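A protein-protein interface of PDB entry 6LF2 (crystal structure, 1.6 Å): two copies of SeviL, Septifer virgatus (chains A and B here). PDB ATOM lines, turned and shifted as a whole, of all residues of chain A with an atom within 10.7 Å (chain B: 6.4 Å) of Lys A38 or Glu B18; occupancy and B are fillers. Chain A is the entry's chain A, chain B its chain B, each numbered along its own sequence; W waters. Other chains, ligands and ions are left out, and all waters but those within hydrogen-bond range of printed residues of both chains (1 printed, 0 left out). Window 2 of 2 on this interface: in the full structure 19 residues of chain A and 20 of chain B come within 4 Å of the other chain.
The backbone carbonyl oxygen (O) of Gly A37 is in hydrogen-bond range of the backbone NH (N) of Gly B20, at 3.4 Å. The side-chain amino group (NZ) of Lys A38 is in salt-bridge range of the side-chain carboxylate (OE1) of Glu B18, at 3.1 Å. The backbone carbonyl oxygen (O) of Arg B17 is in hydrogen-bond range of the backbone NH (N) of Met A39, 2.9 Å away. O of Asn B16 sits close to SD of Met A39.
Tyr A13 touches Phe B95. O of Gly A37 touches C of Asn B19 (3.4 Å). Lys A38 touches Arg B17.
Printed residues of chain B within 4 Å of Tyr A13: Phe B95 (3.6 Å). Ile A14 touches none of the printed residues of chain B. Of the printed residues of chain B, Gly A37 touches Asn B19 and Gly B20. Lys A38 touches two residues of chain B. Printed residues of chain B within 4 Å of Met A39: Asn B16 (3.8 Å) and Arg B17 (2.9 Å). Asn B16 touches just one residue of chain A: Met A39 (3.8 Å). Printed residues of chain A within 4 Å of Glu B18: Lys A38. Of chain A, only Gly A37 (3.4 Å) comes within 4 Å of Asn B19. Printed residues of chain A within 4 Å of Gly B20: Gly A37. No residue of chain A comes within 4 Å of Glu B122. No residue of chain A comes within 4 Å of Ser B123. The nearest residue of chain A that does not touch Glu B18 is Gly A37 (4.5 Å). The nearest printed residue of chain B that does not touch Tyr A13 is Arg B17 (6.1 Å).
Positions printed for both chains: 19, 20 and 21. Of the 7 pairs that touch across the chains among the printed residues, none has its exchanged pair printed and touching as well.
Hydrophobic or aromatic side chains of chain B that line the printed part of chain A: Phe B95. Of the 22 printed residues of chain A, 4 touch a printed residue of chain B. Printed residues of chain A that touch a printed residue of chain B: Tyr A13, Gly A37, Lys A38 and Met A39. Hydrophobic or aromatic side chains of chain A that line the printed part of chain B: Tyr A13 and Met A39. Among the printed residues, Asp or Glu carboxylates within 4 Å of a Lys or Arg side-chain nitrogen of the other chain: Lys A38 with Glu B18 (3.1 Å).
Water W1 lies within hydrogen-bond range of O of Gly B20 (2.6 Å), O of Gly A20 (2.8 Å), NE2 of Gln A15 (3.2 Å) and NH1 of Arg A22 (3.4 Å).
The backbone carbonyl oxygen (O) of Phe A129 lies within hydrogen-bond range of the backbone NH (N) of Tyr A13, 2.9 Å away. O of Gly A37 lies within hydrogen-bond range of NH2 of Arg A22, 2.8 Å away. The guanidinium group of Arg A22 lies within hydrogen-bond range of the backbone carbonyl oxygen of Lys A38 (3.2 Å). The side-chain amide oxygen (OD1) of Asn B16 is in hydrogen-bond range of the backbone NH (N) of Glu B18 (2.8 Å). The side-chain amide nitrogen (ND2) of Asn B16 lies within hydrogen-bond range of the backbone carbonyl oxygen (O) of Ser B123 (2.8 Å). The backbone carbonyl oxygen (O) of Lys B125 is in hydrogen-bond range of the backbone NH (N) of Arg B17 (2.9 Å).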
ATOM      1  N   TYR A  13     -21.964  10.952   6.156  1.00  0.00           N
ATOM      2  CA  TYR A  13     -20.623  10.939   6.716  1.00  0.00           C
ATOM      3  C   TYR A  13     -19.644  11.285   5.605  1.00  0.00           C
ATOM      4  O   TYR A  13     -19.898  11.000   4.433  1.00  0.00           O
ATOM      5  CB  TYR A  13     -20.271   9.561   7.294  1.00  0.00           C
ATOM      6  CG  TYR A  13     -21.132   9.121   8.457  1.00  0.00           C
ATOM      7  CD1 TYR A  13     -20.816   9.507   9.757  1.00  0.00           C
ATOM      8  CD2 TYR A  13     -22.240   8.291   8.262  1.00  0.00           C
ATOM      9  CE1 TYR A  13     -21.593   9.109  10.836  1.00  0.00           C
ATOM     10  CE2 TYR A  13     -23.037   7.882   9.351  1.00  0.00           C
ATOM     11  CZ  TYR A  13     -22.692   8.284  10.633  1.00  0.00           C
ATOM     12  OH  TYR A  13     -23.445   7.908  11.730  1.00  0.00           O
ATOM     13  N   ILE A  14     -18.531  11.922   5.973  1.00  0.00           N
ATOM     14  CA  ILE A  14     -17.523  12.368   5.014  1.00  0.00           C
ATOM     15  C   ILE A  14     -16.201  11.740   5.445  1.00  0.00           C
ATOM     16  O   ILE A  14     -15.590  12.166   6.434  1.00  0.00           O
ATOM     17  CB  ILE A  14     -17.441  13.898   4.952  1.00  0.00           C
ATOM     18  CG1 ILE A  14     -18.816  14.454   4.546  1.00  0.00           C
ATOM     19  CG2 ILE A  14     -16.382  14.321   3.960  1.00  0.00           C
ATOM     20  CD1 ILE A  14     -18.895  15.983   4.527  1.00  0.00           C
ATOM     21  N   GLN A  15     -15.778  10.694   4.727  1.00  0.00           N
ATOM     22  CA  GLN A  15     -14.735   9.781   5.176  1.00  0.00           C
ATOM     23  C   GLN A  15     -13.573   9.760   4.191  1.00  0.00           C
ATOM     24  O   GLN A  15     -13.777   9.746   2.976  1.00  0.00           O
ATOM     25  CB  GLN A  15     -15.304   8.370   5.340  1.00  0.00           C
ATOM     26  CG  GLN A  15     -14.317   7.379   5.894  1.00  0.00           C
ATOM     27  CD  GLN A  15     -15.016   6.194   6.510  1.00  0.00           C
ATOM     28  OE1 GLN A  15     -15.761   6.343   7.473  1.00  0.00           O
ATOM     29  NE2 GLN A  15     -14.794   5.010   5.948  1.00  0.00           N
ATOM     30  N   ASN A  19      -7.027   7.141   5.249  1.00  0.00           N
ATOM     31  CA  ASN A  19      -6.894   6.718   6.636  1.00  0.00           C
ATOM     32  C   ASN A  19      -8.206   6.296   7.284  1.00  0.00           C
ATOM     33  O   ASN A  19      -8.187   5.922   8.461  1.00  0.00           O
ATOM     34  CB  ASN A  19      -6.240   7.831   7.475  1.00  0.00           C
ATOM     35  CG  ASN A  19      -7.187   8.980   7.783  1.00  0.00           C
ATOM     36  OD1 ASN A  19      -8.198   9.169   7.108  1.00  0.00           O
ATOM     37  ND2 ASN A  19      -6.867   9.737   8.828  1.00  0.00           N
ATOM     38  N   GLY A  20      -9.334   6.336   6.567  1.00  0.00           N
ATOM     39  CA  GLY A  20     -10.624   5.986   7.125  1.00  0.00           C
ATOM     40  C   GLY A  20     -11.182   6.970   8.135  1.00  0.00           C
ATOM     41  O   GLY A  20     -12.216   6.683   8.759  1.00  0.00           O
ATOM     42  N   GLY A  21     -10.525   8.122   8.314  1.00  0.00           N
ATOM     43  CA  GLY A  21     -11.007   9.121   9.262  1.00  0.00           C
ATOM     44  C   GLY A  21     -12.197   9.895   8.718  1.00  0.00           C
ATOM     45  O   GLY A  21     -12.397  10.011   7.505  1.00  0.00           O
ATOM     46  N   ARG A  22     -13.016  10.411   9.637  1.00  0.00           N
ATOM     47  CA  ARG A  22     -14.219  11.151   9.270  1.00  0.00           C
ATOM     48  C   ARG A  22     -14.173  12.584   9.783  1.00  0.00           C
ATOM     49  O   ARG A  22     -13.802  12.839  10.936  1.00  0.00           O
ATOM     50  CB  ARG A  22     -15.473  10.449   9.796  1.00  0.00           C
ATOM     51  CG  ARG A  22     -15.884   9.307   8.880  1.00  0.00           C
ATOM     52  CD  ARG A  22     -17.021   8.457   9.451  1.00  0.00           C
ATOM     53  NE  ARG A  22     -16.753   8.179  10.851  1.00  0.00           N
ATOM     54  CZ  ARG A  22     -15.819   7.336  11.280  1.00  0.00           C
ATOM     55  NH1 ARG A  22     -15.097   6.628  10.421  1.00  0.00           N
ATOM     56  NH2 ARG A  22     -15.621   7.204  12.581  1.00  0.00           N
ATOM     57  N   ALA A  23     -14.573  13.521   8.922  1.00  0.00           N
ATOM     58  CA  ALA A  23     -14.710  14.907   9.349  1.00  0.00           C
ATOM     59  C   ALA A  23     -15.787  15.030  10.420  1.00  0.00           C
ATOM     60  O   ALA A  23     -16.788  14.314  10.392  1.00  0.00           O
ATOM     61  CB  ALA A  23     -15.050  15.780   8.141  1.00  0.00           C
ATOM     62  N   PHE A  24     -15.567  15.927  11.383  1.00  0.00           N
ATOM     63  CA  PHE A  24     -16.558  16.162  12.427  1.00  0.00           C
ATOM     64  C   PHE A  24     -16.519  17.621  12.852  1.00  0.00           C
ATOM     65  O   PHE A  24     -15.522  18.321  12.654  1.00  0.00           O
ATOM     66  CB  PHE A  24     -16.320  15.276  13.654  1.00  0.00           C
ATOM     67  CG  PHE A  24     -15.151  15.722  14.495  1.00  0.00           C
ATOM     68  CD1 PHE A  24     -13.859  15.308  14.185  1.00  0.00           C
ATOM     69  CD2 PHE A  24     -15.340  16.560  15.585  1.00  0.00           C
ATOM     70  CE1 PHE A  24     -12.778  15.727  14.951  1.00  0.00           C
ATOM     71  CE2 PHE A  24     -14.259  16.990  16.353  1.00  0.00           C
ATOM     72  CZ  PHE A  24     -12.985  16.575  16.041  1.00  0.00           C
ATOM     73  N   ARG A  29     -17.553  21.856  22.105  1.00  0.00           N
ATOM     74  CA  ARG A  29     -16.108  21.969  22.260  1.00  0.00           C
ATOM     75  C   ARG A  29     -15.471  22.953  21.288  1.00  0.00           C
ATOM     76  O   ARG A  29     -14.257  23.200  21.388  1.00  0.00           O
ATOM     77  CB  ARG A  29     -15.442  20.600  22.083  1.00  0.00           C
ATOM     78  CG  ARG A  29     -15.871  19.542  23.069  1.00  0.00           C
ATOM     79  CD  ARG A  29     -14.771  18.476  23.203  1.00  0.00           C
ATOM     80  NE  ARG A  29     -14.286  18.008  21.899  1.00  0.00           N
ATOM     81  CZ  ARG A  29     -14.863  17.043  21.183  1.00  0.00           C
ATOM     82  NH1 ARG A  29     -15.954  16.437  21.636  1.00  0.00           N
ATOM     83  NH2 ARG A  29     -14.350  16.691  20.004  1.00  0.00           N
ATOM     84  N   ILE A  34     -10.798  15.935  11.956  1.00  0.00           N
ATOM     85  CA  ILE A  34     -10.995  14.609  11.390  1.00  0.00           C
ATOM     86  C   ILE A  34     -10.656  13.604  12.479  1.00  0.00           C
ATOM     87  O   ILE A  34      -9.752  13.839  13.288  1.00  0.00           O
ATOM     88  CB  ILE A  34     -10.152  14.390  10.113  1.00  0.00           C
ATOM     89  CG1 ILE A  34     -10.436  13.016   9.509  1.00  0.00           C
ATOM     90  CG2 ILE A  34      -8.661  14.606  10.380  1.00  0.00           C
ATOM     91  CD1 ILE A  34      -9.729  12.759   8.183  1.00  0.00           C
ATOM     92  N   PHE A  35     -11.403  12.507  12.527  1.00  0.00           N
ATOM     93  CA  PHE A  35     -11.308  11.572  13.642  1.00  0.00           C
ATOM     94  C   PHE A  35     -11.294  10.137  13.137  1.00  0.00           C
ATOM     95  O   PHE A  35     -12.083   9.774  12.260  1.00  0.00           O
ATOM     96  CB  PHE A  35     -12.493  11.793  14.595  1.00  0.00           C
ATOM     97  CG  PHE A  35     -12.566  10.830  15.739  1.00  0.00           C
ATOM     98  CD1 PHE A  35     -11.772  11.007  16.861  1.00  0.00           C
ATOM     99  CD2 PHE A  35     -13.464   9.766  15.713  1.00  0.00           C
ATOM    100  CE1 PHE A  35     -11.875  10.131  17.939  1.00  0.00           C
ATOM    101  CE2 PHE A  35     -13.566   8.896  16.771  1.00  0.00           C
ATOM    102  CZ  PHE A  35     -12.770   9.072  17.888  1.00  0.00           C
ATOM    103  N   THR A  36     -10.400   9.325  13.702  1.00  0.00           N
ATOM    104  CA  THR A  36     -10.410   7.890  13.461  1.00  0.00           C
ATOM    105  C   THR A  36     -10.977   7.174  14.679  1.00  0.00           C
ATOM    106  O   THR A  36     -10.598   7.464  15.821  1.00  0.00           O
ATOM    107  CB  THR A  36      -9.013   7.351  13.140  1.00  0.00           C
ATOM    108  OG1 THR A  36      -8.083   7.732  14.155  1.00  0.00           O
ATOM    109  CG2 THR A  36      -8.542   7.860  11.831  1.00  0.00           C
ATOM    110  N   GLY A  37     -11.895   6.259  14.430  1.00  0.00           N
ATOM    111  CA  GLY A  37     -12.463   5.474  15.497  1.00  0.00           C
ATOM    112  C   GLY A  37     -13.974   5.421  15.434  1.00  0.00           C
ATOM    113  O   GLY A  37     -14.566   5.348  14.352  1.00  0.00           O
ATOM    114  N   LYS A  38     -14.594   5.483  16.606  1.00  0.00           N
ATOM    115  CA  LYS A  38     -16.034   5.332  16.738  1.00  0.00           C
ATOM    116  C   LYS A  38     -16.790   6.357  15.891  1.00  0.00           C
ATOM    117  O   LYS A  38     -16.351   7.493  15.722  1.00  0.00           O
ATOM    118  CB  LYS A  38     -16.412   5.461  18.217  1.00  0.00           C
ATOM    119  CG  LYS A  38     -17.875   5.271  18.514  1.00  0.00           C
ATOM    120  CD  LYS A  38     -18.098   4.897  19.964  1.00  0.00           C
ATOM    121  CE  LYS A  38     -19.592   4.802  20.267  1.00  0.00           C
ATOM    122  NZ  LYS A  38     -19.820   4.026  21.519  1.00  0.00           N
ATOM    123  N   MET A  39     -17.960   5.949  15.380  1.00  0.00           N
ATOM    124  CA  MET A  39     -18.781   6.803  14.517  1.00  0.00           C
ATOM    125  C   MET A  39     -19.763   7.606  15.369  1.00  0.00           C
ATOM    126  O   MET A  39     -20.944   7.283  15.485  1.00  0.00           O
ATOM    127  CB  MET A  39     -19.511   5.959  13.476  1.00  0.00           C
ATOM    128  CG  MET A  39     -18.578   5.108  12.633  1.00  0.00           C
ATOM    129  SD  MET A  39     -19.402   4.280  11.256  1.00  0.00           S
ATOM    130  CE  MET A  39     -19.914   5.692  10.268  1.00  0.00           C
ATOM    131  N   TYR A  40     -19.261   8.696  15.953  1.00  0.00           N
ATOM    132  CA  TYR A  40     -20.069   9.576  16.793  1.00  0.00           C
ATOM    133  C   TYR A  40     -20.994  10.452  15.951  1.00  0.00           C
ATOM    134  O   TYR A  40     -20.748  10.705  14.768  1.00  0.00           O
ATOM    135  CB  TYR A  40     -19.173  10.467  17.651  1.00  0.00           C
ATOM    136  CG  TYR A  40     -18.404   9.732  18.726  1.00  0.00           C
ATOM    137  CD1 TYR A  40     -19.062   9.170  19.819  1.00  0.00           C
ATOM    138  CD2 TYR A  40     -17.023   9.640  18.670  1.00  0.00           C
ATOM    139  CE1 TYR A  40     -18.358   8.507  20.808  1.00  0.00           C
ATOM    140  CE2 TYR A  40     -16.310   8.991  19.658  1.00  0.00           C
ATOM    141  CZ  TYR A  40     -16.984   8.421  20.724  1.00  0.00           C
ATOM    142  OH  TYR A  40     -16.270   7.764  21.710  1.00  0.00           O
ATOM    143  N   ASP A  41     -22.056  10.951  16.591  1.00  0.00           N
ATOM    144  CA  ASP A  41     -23.052  11.704  15.841  1.00  0.00           C
ATOM    145  C   ASP A  41     -22.544  13.076  15.402  1.00  0.00           C
ATOM    146  O   ASP A  41     -23.115  13.657  14.470  1.00  0.00           O
ATOM    147  CB  ASP A  41     -24.347  11.840  16.647  1.00  0.00           C
ATOM    148  CG  ASP A  41     -24.318  13.004  17.604  1.00  0.00           C
ATOM    149  OD1 ASP A  41     -23.422  13.033  18.473  1.00  0.00           O
ATOM    150  OD2 ASP A  41     -25.184  13.904  17.476  1.00  0.00           O
ATOM    151  N   ASP A  42     -21.468  13.596  16.000  1.00  0.00           N
ATOM    152  CA  ASP A  42     -20.934  14.855  15.484  1.00  0.00           C
ATOM    153  C   ASP A  42     -20.172  14.672  14.166  1.00  0.00           C
ATOM    154  O   ASP A  42     -19.587  15.636  13.656  1.00  0.00           O
ATOM    155  CB  ASP A  42     -20.079  15.585  16.545  1.00  0.00           C
ATOM    156  CG  ASP A  42     -18.834  14.825  16.990  1.00  0.00           C
ATOM    157  OD1 ASP A  42     -18.441  13.835  16.345  1.00  0.00           O
ATOM    158  OD2 ASP A  42     -18.255  15.244  18.020  1.00  0.00           O
ATOM    159  N   GLN A  43     -20.211  13.470  13.585  1.00  0.00           N
ATOM    160  CA  GLN A  43     -19.653  13.207  12.269  1.00  0.00           C
ATOM    161  C   GLN A  43     -20.714  13.207  11.172  1.00  0.00           C
ATOM    162  O   GLN A  43     -20.386  12.920  10.017  1.00  0.00           O
ATOM    163  CB  GLN A  43     -18.902  11.863  12.291  1.00  0.00           C
ATOM    164  CG  GLN A  43     -17.683  11.860  13.218  1.00  0.00           C
ATOM    165  CD  GLN A  43     -17.285  10.452  13.667  1.00  0.00           C
ATOM    166  OE1 GLN A  43     -17.612   9.458  13.017  1.00  0.00           O
ATOM    167  NE2 GLN A  43     -16.607  10.369  14.804  1.00  0.00           N
ATOM    168  N   ILE A  44     -21.972  13.530  11.494  1.00  0.00           N
ATOM    169  CA  ILE A  44     -23.048  13.537  10.499  1.00  0.00           C
ATOM    170  C   ILE A  44     -23.212  14.954   9.954  1.00  0.00           C
ATOM    171  O   ILE A  44     -23.569  15.881  10.696  1.00  0.00           O
ATOM    172  CB  ILE A  44     -24.366  13.025  11.094  1.00  0.00           C
ATOM    173  CG1 ILE A  44     -24.213  11.580  11.573  1.00  0.00           C
ATOM    174  CG2 ILE A  44     -25.478  13.110  10.059  1.00  0.00           C
ATOM    175  CD1 ILE A  44     -25.380  11.078  12.393  1.00  0.00           C
ATOM    176  N   PHE A 129     -21.108   9.271   2.281  1.00  0.00           N
ATOM    177  CA  PHE A 129     -22.125   8.231   2.255  1.00  0.00           C
ATOM    178  C   PHE A 129     -23.295   8.539   3.183  1.00  0.00           C
ATOM    179  O   PHE A 129     -23.157   9.194   4.218  1.00  0.00           O
ATOM    180  CB  PHE A 129     -21.526   6.833   2.559  1.00  0.00           C
ATOM    181  CG  PHE A 129     -20.837   6.695   3.903  1.00  0.00           C
ATOM    182  CD1 PHE A 129     -21.534   6.208   5.006  1.00  0.00           C
ATOM    183  CD2 PHE A 129     -19.473   6.951   4.044  1.00  0.00           C
ATOM    184  CE1 PHE A 129     -20.894   6.018   6.234  1.00  0.00           C
ATOM    185  CE2 PHE A 129     -18.841   6.782   5.271  1.00  0.00           C
ATOM    186  CZ  PHE A 129     -19.547   6.297   6.362  1.00  0.00           C
ATOM    187  N   ASN B  16     -18.187  -0.780  10.944  1.00  0.00           N
ATOM    188  CA  ASN B  16     -18.663  -0.919  12.312  1.00  0.00           C
ATOM    189  C   ASN B  16     -18.786   0.435  12.995  1.00  0.00           C
ATOM    190  O   ASN B  16     -17.880   1.268  12.914  1.00  0.00           O
ATOM    191  CB  ASN B  16     -17.701  -1.802  13.108  1.00  0.00           C
ATOM    192  CG  ASN B  16     -18.352  -2.391  14.338  1.00  0.00           C
ATOM    193  OD1 ASN B  16     -18.420  -1.750  15.391  1.00  0.00           O
ATOM    194  ND2 ASN B  16     -18.854  -3.616  14.210  1.00  0.00           N
ATOM    195  N   ARG B  17     -19.900   0.629  13.708  1.00  0.00           N
ATOM    196  CA  ARG B  17     -20.092   1.871  14.458  1.00  0.00           C
ATOM    197  C   ARG B  17     -19.047   2.055  15.553  1.00  0.00           C
ATOM    198  O   ARG B  17     -18.667   3.192  15.867  1.00  0.00           O
ATOM    199  CB  ARG B  17     -21.483   1.899  15.081  1.00  0.00           C
ATOM    200  CG  ARG B  17     -21.836   3.242  15.734  1.00  0.00           C
ATOM    201  CD  ARG B  17     -23.297   3.236  16.124  1.00  0.00           C
ATOM    202  NE  ARG B  17     -23.694   4.464  16.807  1.00  0.00           N
ATOM    203  CZ  ARG B  17     -23.486   4.696  18.100  1.00  0.00           C
ATOM    204  NH1 ARG B  17     -22.874   3.785  18.846  1.00  0.00           N
ATOM    205  NH2 ARG B  17     -23.887   5.837  18.644  1.00  0.00           N
ATOM    206  N   GLU B  18     -18.601   0.964  16.185  1.00  0.00           N
ATOM    207  CA  GLU B  18     -17.838   1.116  17.417  1.00  0.00           C
ATOM    208  C   GLU B  18     -16.383   1.509  17.180  1.00  0.00           C
ATOM    209  O   GLU B  18     -15.810   2.229  18.006  1.00  0.00           O
ATOM    210  CB  GLU B  18     -17.937  -0.178  18.234  1.00  0.00           C
ATOM    211  CG  GLU B  18     -17.309  -0.106  19.613  1.00  0.00           C
ATOM    212  CD  GLU B  18     -18.095   0.754  20.595  1.00  0.00           C
ATOM    213  OE1 GLU B  18     -19.200   1.228  20.259  1.00  0.00           O
ATOM    214  OE2 GLU B  18     -17.597   0.953  21.722  1.00  0.00           O
ATOM    215  N   ASN B  19     -15.771   1.076  16.068  1.00  0.00           N
ATOM    216  CA  ASN B  19     -14.388   1.414  15.775  1.00  0.00           C
ATOM    217  C   ASN B  19     -14.155   1.953  14.367  1.00  0.00           C
ATOM    218  O   ASN B  19     -13.000   2.207  14.006  1.00  0.00           O
ATOM    219  CB  ASN B  19     -13.486   0.191  15.998  1.00  0.00           C
ATOM    220  CG  ASN B  19     -13.783  -0.947  15.036  1.00  0.00           C
ATOM    221  OD1 ASN B  19     -14.675  -0.856  14.193  1.00  0.00           O
ATOM    222  ND2 ASN B  19     -13.027  -2.030  15.161  1.00  0.00           N
ATOM    223  N   GLY B  20     -15.204   2.152  13.573  1.00  0.00           N
ATOM    224  CA  GLY B  20     -15.054   2.598  12.199  1.00  0.00           C
ATOM    225  C   GLY B  20     -14.384   1.610  11.272  1.00  0.00           C
ATOM    226  O   GLY B  20     -14.031   1.983  10.147  1.00  0.00           O
ATOM    227  N   GLY B  21     -14.195   0.364  11.713  1.00  0.00           N
ATOM    228  CA  GLY B  21     -13.503  -0.619  10.895  1.00  0.00           C
ATOM    229  C   GLY B  21     -14.391  -1.266   9.849  1.00  0.00           C
ATOM    230  O   GLY B  21     -15.605  -1.422  10.020  1.00  0.00           O
ATOM    231  N   PHE B  95     -28.008   2.254  11.182  1.00  0.00           N
ATOM    232  CA  PHE B  95     -27.212   1.089  11.539  1.00  0.00           C
ATOM    233  C   PHE B  95     -28.081  -0.155  11.670  1.00  0.00           C
ATOM    234  O   PHE B  95     -29.272  -0.080  11.983  1.00  0.00           O
ATOM    235  CB  PHE B  95     -26.441   1.333  12.838  1.00  0.00           C
ATOM    236  CG  PHE B  95     -25.315   2.320  12.675  1.00  0.00           C
ATOM    237  CD1 PHE B  95     -25.556   3.677  12.764  1.00  0.00           C
ATOM    238  CD2 PHE B  95     -24.027   1.888  12.390  1.00  0.00           C
ATOM    239  CE1 PHE B  95     -24.532   4.588  12.601  1.00  0.00           C
ATOM    240  CE2 PHE B  95     -22.997   2.803  12.220  1.00  0.00           C
ATOM    241  CZ  PHE B  95     -23.255   4.153  12.329  1.00  0.00           C
ATOM    242  N   TYR B 109     -17.050  -8.384  16.092  1.00  0.00           N
ATOM    243  CA  TYR B 109     -15.618  -8.497  15.875  1.00  0.00           C
ATOM    244  C   TYR B 109     -14.909  -8.705  17.206  1.00  0.00           C
ATOM    245  O   TYR B 109     -15.433  -8.396  18.280  1.00  0.00           O
ATOM    246  CB  TYR B 109     -15.046  -7.277  15.117  1.00  0.00           C
ATOM    247  CG  TYR B 109     -15.077  -5.967  15.887  1.00  0.00           C
ATOM    248  CD1 TYR B 109     -14.027  -5.605  16.726  1.00  0.00           C
ATOM    249  CD2 TYR B 109     -16.149  -5.089  15.767  1.00  0.00           C
ATOM    250  CE1 TYR B 109     -14.050  -4.419  17.437  1.00  0.00           C
ATOM    251  CE2 TYR B 109     -16.180  -3.901  16.476  1.00  0.00           C
ATOM    252  CZ  TYR B 109     -15.127  -3.571  17.306  1.00  0.00           C
ATOM    253  OH  TYR B 109     -15.142  -2.386  18.014  1.00  0.00           O
ATOM    254  N   GLU B 122     -22.506  -3.729  21.746  1.00  0.00           N
ATOM    255  CA  GLU B 122     -22.315  -2.459  21.055  1.00  0.00           C
ATOM    256  C   GLU B 122     -21.481  -2.594  19.777  1.00  0.00           C
ATOM    257  O   GLU B 122     -21.608  -1.760  18.873  1.00  0.00           O
ATOM    258  CB  GLU B 122     -21.675  -1.465  22.027  1.00  0.00           C
ATOM    259  CG  GLU B 122     -22.006  -0.011  21.796  1.00  0.00           C
ATOM    260  CD  GLU B 122     -23.503   0.294  21.761  1.00  0.00           C
ATOM    261  OE1 GLU B 122     -24.308  -0.389  22.440  1.00  0.00           O
ATOM    262  OE2 GLU B 122     -23.868   1.237  21.036  1.00  0.00           O
ATOM    263  N   SER B 123     -20.642  -3.626  19.663  1.00  0.00           N
ATOM    264  CA  SER B 123     -19.797  -3.818  18.489  1.00  0.00           C
ATOM    265  C   SER B 123     -20.466  -4.650  17.387  1.00  0.00           C
ATOM    266  O   SER B 123     -19.788  -5.073  16.444  1.00  0.00           O
ATOM    267  CB  SER B 123     -18.485  -4.470  18.910  1.00  0.00           C
ATOM    268  OG  SER B 123     -18.757  -5.518  19.816  1.00  0.00           O
ATOM    269  N   GLU B 124     -21.774  -4.878  17.475  1.00  0.00           N
ATOM    270  CA  GLU B 124     -22.535  -5.559  16.438  1.00  0.00           C
ATOM    271  C   GLU B 124     -23.255  -4.606  15.500  1.00  0.00           C
ATOM    272  O   GLU B 124     -24.064  -5.062  14.677  1.00  0.00           O
ATOM    273  CB  GLU B 124     -23.568  -6.497  17.074  1.00  0.00           C
ATOM    274  CG  GLU B 124     -22.936  -7.609  17.880  1.00  0.00           C
ATOM    275  CD  GLU B 124     -23.907  -8.272  18.825  1.00  0.00           C
ATOM    276  OE1 GLU B 124     -25.013  -7.729  19.030  1.00  0.00           O
ATOM    277  OE2 GLU B 124     -23.553  -9.352  19.354  1.00  0.00           O
ATOM    278  N   LYS B 125     -23.027  -3.290  15.627  1.00  0.00           N
ATOM    279  CA  LYS B 125     -23.770  -2.302  14.852  1.00  0.00           C
ATOM    280  C   LYS B 125     -22.966  -1.931  13.614  1.00  0.00           C
ATOM    281  O   LYS B 125     -21.820  -1.483  13.731  1.00  0.00           O
ATOM    282  CB  LYS B 125     -24.067  -1.068  15.703  1.00  0.00           C
ATOM    283  CG  LYS B 125     -24.901  -1.371  16.938  1.00  0.00           C
ATOM    284  CD  LYS B 125     -25.072  -0.151  17.818  1.00  0.00           C
ATOM    285  CE  LYS B 125     -25.942  -0.481  19.015  1.00  0.00           C
ATOM    286  NZ  LYS B 125     -26.199   0.729  19.865  1.00  0.00           N
HETATM  287  O   HOH W   1     -13.517   4.164   8.758  1.00  0.00           O
